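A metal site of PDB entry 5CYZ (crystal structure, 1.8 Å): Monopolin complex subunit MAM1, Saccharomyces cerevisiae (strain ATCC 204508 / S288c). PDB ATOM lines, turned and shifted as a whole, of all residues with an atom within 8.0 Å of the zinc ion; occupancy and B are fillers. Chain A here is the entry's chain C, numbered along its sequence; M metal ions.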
ATOM      1  N   ILE A  26       4.812   9.950  23.363  1.00  0.00           N
ATOM      2  CA  ILE A  26       4.268  10.806  22.322  1.00  0.00           C
ATOM      3  C   ILE A  26       2.923  10.225  21.887  1.00  0.00           C
ATOM      4  O   ILE A  26       2.844   9.282  21.093  1.00  0.00           O
ATOM      5  CB  ILE A  26       5.242  10.966  21.154  1.00  0.00           C
ATOM      6  CG1 ILE A  26       6.562  11.554  21.679  1.00  0.00           C
ATOM      7  CG2 ILE A  26       4.646  11.904  20.102  1.00  0.00           C
ATOM      8  CD1 ILE A  26       7.643  11.676  20.622  1.00  0.00           C
ATOM      9  N   ALA A  27       1.854  10.796  22.421  1.00  0.00           N
ATOM     10  CA  ALA A  27       0.574  10.108  22.452  1.00  0.00           C
ATOM     11  C   ALA A  27      -0.395  10.541  21.347  1.00  0.00           C
ATOM     12  O   ALA A  27      -1.587  10.251  21.403  1.00  0.00           O
ATOM     13  CB  ALA A  27      -0.079  10.297  23.815  1.00  0.00           C
ATOM     14  N   CYS A  28       0.123  11.220  20.329  1.00  0.00           N
ATOM     15  CA  CYS A  28      -0.689  11.576  19.189  1.00  0.00           C
ATOM     16  C   CYS A  28      -0.937  10.327  18.334  1.00  0.00           C
ATOM     17  O   CYS A  28      -0.451   9.253  18.645  1.00  0.00           O
ATOM     18  CB  CYS A  28       0.012  12.651  18.358  1.00  0.00           C
ATOM     19  SG  CYS A  28       1.456  11.989  17.615  1.00  0.00           S
ATOM     20  N   ASP A  29      -1.672  10.477  17.233  1.00  0.00           N
ATOM     21  CA  ASP A  29      -1.888   9.342  16.349  1.00  0.00           C
ATOM     22  C   ASP A  29      -1.325   9.601  14.951  1.00  0.00           C
ATOM     23  O   ASP A  29      -1.734   8.952  13.994  1.00  0.00           O
ATOM     24  CB  ASP A  29      -3.386   9.018  16.262  1.00  0.00           C
ATOM     25  CG  ASP A  29      -3.912   8.371  17.536  1.00  0.00           C
ATOM     26  OD1 ASP A  29      -3.157   7.587  18.164  1.00  0.00           O
ATOM     27  OD2 ASP A  29      -5.064   8.647  17.915  1.00  0.00           O
ATOM     28  N   HIS A  30      -0.373  10.524  14.843  1.00  0.00           N
ATOM     29  CA  HIS A  30       0.229  10.829  13.553  1.00  0.00           C
ATOM     30  C   HIS A  30       1.186   9.737  13.094  1.00  0.00           C
ATOM     31  O   HIS A  30       1.989   9.263  13.880  1.00  0.00           O
ATOM     32  CB  HIS A  30       0.982  12.163  13.643  1.00  0.00           C
ATOM     33  CG  HIS A  30       0.116  13.291  14.134  1.00  0.00           C
ATOM     34  ND1 HIS A  30       0.557  14.194  15.074  1.00  0.00           N
ATOM     35  CD2 HIS A  30      -1.161  13.634  13.831  1.00  0.00           C
ATOM     36  CE1 HIS A  30      -0.422  15.053  15.325  1.00  0.00           C
ATOM     37  NE2 HIS A  30      -1.462  14.739  14.585  1.00  0.00           N
ATOM     38  N   CYS A  31       1.087   9.360  11.825  1.00  0.00           N
ATOM     39  CA  CYS A  31       1.951   8.308  11.294  1.00  0.00           C
ATOM     40  C   CYS A  31       3.433   8.676  11.421  1.00  0.00           C
ATOM     41  O   CYS A  31       4.259   7.842  11.820  1.00  0.00           O
ATOM     42  CB  CYS A  31       1.615   8.022   9.829  1.00  0.00           C
ATOM     43  SG  CYS A  31      -0.019   7.297   9.596  1.00  0.00           S
ATOM     44  N   LEU A  32       3.774   9.928  11.129  1.00  0.00           N
ATOM     45  CA  LEU A  32       5.174  10.316  11.161  1.00  0.00           C
ATOM     46  C   LEU A  32       5.758  10.354  12.567  1.00  0.00           C
ATOM     47  O   LEU A  32       6.945  10.133  12.752  1.00  0.00           O
ATOM     48  CB  LEU A  32       5.365  11.677  10.497  1.00  0.00           C
ATOM     49  CG  LEU A  32       5.122  11.694   8.981  1.00  0.00           C
ATOM     50  CD1 LEU A  32       5.374  13.092   8.447  1.00  0.00           C
ATOM     51  CD2 LEU A  32       5.998  10.660   8.284  1.00  0.00           C
ATOM     52  N   CYS A  33       4.925  10.671  13.554  1.00  0.00           N
ATOM     53  CA  CYS A  33       5.368  10.720  14.950  1.00  0.00           C
ATOM     54  C   CYS A  33       5.522   9.327  15.580  1.00  0.00           C
ATOM     55  O   CYS A  33       6.198   9.181  16.601  1.00  0.00           O
ATOM     56  CB  CYS A  33       4.372  11.531  15.790  1.00  0.00           C
ATOM     57  SG  CYS A  33       4.236  13.263  15.339  1.00  0.00           S
ATOM     58  N   SER A  34       4.898   8.338  14.957  1.00  0.00           N
ATOM     59  CA  SER A  34       4.674   7.038  15.592  1.00  0.00           C
ATOM     60  C   SER A  34       5.949   6.239  15.805  1.00  0.00           C
ATOM     61  O   SER A  34       6.945   6.448  15.116  1.00  0.00           O
ATOM     62  CB  SER A  34       3.690   6.206  14.763  1.00  0.00           C
ATOM     63  OG  SER A  34       4.295   5.767  13.553  1.00  0.00           O
ATOM     64  N   TRP A  47      14.428  11.634  11.430  1.00  0.00           N
ATOM     65  CA  TRP A  47      13.113  11.734  12.066  1.00  0.00           C
ATOM     66  C   TRP A  47      12.975  13.121  12.696  1.00  0.00           C
ATOM     67  O   TRP A  47      12.161  13.915  12.286  1.00  0.00           O
ATOM     68  CB  TRP A  47      12.918  10.635  13.121  1.00  0.00           C
ATOM     69  CG  TRP A  47      11.556  10.689  13.790  1.00  0.00           C
ATOM     70  CD1 TRP A  47      10.349  10.428  13.203  1.00  0.00           C
ATOM     71  CD2 TRP A  47      11.286  11.057  15.145  1.00  0.00           C
ATOM     72  NE1 TRP A  47       9.340  10.605  14.118  1.00  0.00           N
ATOM     73  CE2 TRP A  47       9.888  10.984  15.319  1.00  0.00           C
ATOM     74  CE3 TRP A  47      12.088  11.414  16.231  1.00  0.00           C
ATOM     75  CZ2 TRP A  47       9.265  11.262  16.543  1.00  0.00           C
ATOM     76  CZ3 TRP A  47      11.460  11.686  17.461  1.00  0.00           C
ATOM     77  CH2 TRP A  47      10.070  11.615  17.599  1.00  0.00           C
ATOM     78  N   LEU A  52       9.877  15.353  11.157  1.00  0.00           N
ATOM     79  CA  LEU A  52       9.086  16.197  12.072  1.00  0.00           C
ATOM     80  C   LEU A  52       9.006  17.680  11.624  1.00  0.00           C
ATOM     81  O   LEU A  52       8.406  18.482  12.323  1.00  0.00           O
ATOM     82  CB  LEU A  52       9.615  16.126  13.512  1.00  0.00           C
ATOM     83  CG  LEU A  52       9.519  14.743  14.205  1.00  0.00           C
ATOM     84  CD1 LEU A  52       9.925  14.850  15.683  1.00  0.00           C
ATOM     85  CD2 LEU A  52       8.118  14.165  14.087  1.00  0.00           C
ATOM     86  N   GLU A  56       0.884  18.623  10.324  1.00  0.00           N
ATOM     87  CA  GLU A  56      -0.441  18.034  10.232  1.00  0.00           C
ATOM     88  C   GLU A  56      -1.560  19.090  10.220  1.00  0.00           C
ATOM     89  O   GLU A  56      -2.538  18.944   9.471  1.00  0.00           O
ATOM     90  CB  GLU A  56      -0.655  17.065  11.398  1.00  0.00           C
ATOM     91  CG  GLU A  56       0.062  15.716  11.252  1.00  0.00           C
ATOM     92  CD  GLU A  56      -0.752  14.696  10.465  1.00  0.00           C
ATOM     93  OE1 GLU A  56      -1.871  15.039  10.017  1.00  0.00           O
ATOM     94  OE2 GLU A  56      -0.271  13.541  10.297  1.00  0.00           O
ATOM     95  N   ASN A  61       4.841  22.767  12.892  1.00  0.00           N
ATOM     96  CA  ASN A  61       5.402  21.484  12.524  1.00  0.00           C
ATOM     97  C   ASN A  61       5.201  20.519  13.687  1.00  0.00           C
ATOM     98  O   ASN A  61       4.731  20.920  14.764  1.00  0.00           O
ATOM     99  CB  ASN A  61       6.884  21.580  12.074  1.00  0.00           C
ATOM    100  CG  ASN A  61       7.843  22.017  13.185  1.00  0.00           C
ATOM    101  OD1 ASN A  61       7.588  21.846  14.377  1.00  0.00           O
ATOM    102  ND2 ASN A  61       8.983  22.578  12.767  1.00  0.00           N
ATOM    103  N   LEU A  62       5.512  19.239  13.464  1.00  0.00           N
ATOM    104  CA  LEU A  62       5.259  18.188  14.448  1.00  0.00           C
ATOM    105  C   LEU A  62       6.285  18.248  15.594  1.00  0.00           C
ATOM    106  O   LEU A  62       5.992  17.816  16.704  1.00  0.00           O
ATOM    107  CB  LEU A  62       5.290  16.811  13.786  1.00  0.00           C
ATOM    108  CG  LEU A  62       4.234  16.574  12.691  1.00  0.00           C
ATOM    109  CD1 LEU A  62       4.596  15.329  11.875  1.00  0.00           C
ATOM    110  CD2 LEU A  62       2.846  16.419  13.314  1.00  0.00           C
ATOM    111  N   ARG A  63       7.471  18.785  15.317  1.00  0.00           N
ATOM    112  CA  ARG A  63       8.463  18.952  16.384  1.00  0.00           C
ATOM    113  C   ARG A  63       7.886  19.899  17.438  1.00  0.00           C
ATOM    114  O   ARG A  63       8.123  19.721  18.627  1.00  0.00           O
ATOM    115  CB  ARG A  63       9.807  19.478  15.853  1.00  0.00           C
ATOM    116  CG  ARG A  63      10.903  19.461  16.936  1.00  0.00           C
ATOM    117  CD  ARG A  63      12.318  19.505  16.340  1.00  0.00           C
ATOM    118  NE  ARG A  63      12.571  20.756  15.640  1.00  0.00           N
ATOM    119  CZ  ARG A  63      12.604  20.877  14.319  1.00  0.00           C
ATOM    120  NH1 ARG A  63      12.422  19.813  13.559  1.00  0.00           N
ATOM    121  NH2 ARG A  63      12.826  22.069  13.768  1.00  0.00           N
ATOM    122  N   SER A  65       4.272  20.796  17.552  1.00  0.00           N
ATOM    123  CA  SER A  65       2.915  20.418  17.952  1.00  0.00           C
ATOM    124  C   SER A  65       2.910  19.156  18.806  1.00  0.00           C
ATOM    125  O   SER A  65       2.038  18.990  19.656  1.00  0.00           O
ATOM    126  CB  SER A  65       2.007  20.242  16.729  1.00  0.00           C
ATOM    127  OG  SER A  65       2.348  19.087  15.973  1.00  0.00           O
ATOM    128  N   CYS A  66       3.898  18.292  18.601  1.00  0.00           N
ATOM    129  CA  CYS A  66       3.892  16.991  19.276  1.00  0.00           C
ATOM    130  C   CYS A  66       5.127  16.745  20.127  1.00  0.00           C
ATOM    131  O   CYS A  66       5.004  16.426  21.312  1.00  0.00           O
ATOM    132  CB  CYS A  66       3.728  15.863  18.255  1.00  0.00           C
ATOM    133  SG  CYS A  66       2.119  15.876  17.401  1.00  0.00           S
ATOM    134  N   TYR A  67       6.317  16.884  19.551  1.00  0.00           N
ATOM    135  CA  TYR A  67       7.499  16.593  20.360  1.00  0.00           C
ATOM    136  C   TYR A  67       7.585  17.542  21.545  1.00  0.00           C
ATOM    137  O   TYR A  67       7.759  17.104  22.678  1.00  0.00           O
ATOM    138  CB  TYR A  67       8.792  16.667  19.534  1.00  0.00           C
ATOM    139  CG  TYR A  67       9.960  16.002  20.255  1.00  0.00           C
ATOM    140  CD1 TYR A  67      10.692  16.677  21.211  1.00  0.00           C
ATOM    141  CD2 TYR A  67      10.306  14.681  19.977  1.00  0.00           C
ATOM    142  CE1 TYR A  67      11.761  16.054  21.873  1.00  0.00           C
ATOM    143  CE2 TYR A  67      11.374  14.048  20.616  1.00  0.00           C
ATOM    144  CZ  TYR A  67      12.087  14.734  21.568  1.00  0.00           C
ATOM    145  OH  TYR A  67      13.128  14.092  22.211  1.00  0.00           O
ATOM    146  N   TYR A  70       4.787  16.608  24.238  1.00  0.00           N
ATOM    147  CA  TYR A  70       4.851  15.359  24.987  1.00  0.00           C
ATOM    148  C   TYR A  70       6.193  15.102  25.638  1.00  0.00           C
ATOM    149  O   TYR A  70       6.285  14.290  26.552  1.00  0.00           O
ATOM    150  CB  TYR A  70       4.478  14.187  24.086  1.00  0.00           C
ATOM    151  CG  TYR A  70       3.028  14.201  23.701  1.00  0.00           C
ATOM    152  CD1 TYR A  70       2.053  13.867  24.635  1.00  0.00           C
ATOM    153  CD2 TYR A  70       2.619  14.577  22.434  1.00  0.00           C
ATOM    154  CE1 TYR A  70       0.717  13.887  24.315  1.00  0.00           C
ATOM    155  CE2 TYR A  70       1.279  14.604  22.103  1.00  0.00           C
ATOM    156  CZ  TYR A  70       0.328  14.253  23.053  1.00  0.00           C
ATOM    157  OH  TYR A  70      -1.006  14.274  22.750  1.00  0.00           O
HETATM  158 ZN    ZN M   1       2.149  13.837  16.317  1.00  0.00          ZN
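SG of Cys 66 sits close to OG of Ser 65, 3.5 Å away.
The zinc ion is bound by a ring nitrogen (ND1) of His 30, the side-chain sulfur (SG) of Cys 66, the side-chain sulfur (SG) of Cys 28 and the side-chain sulfur (SG) of Cys 33.
The zinc ion has four donor atoms within binding distance.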
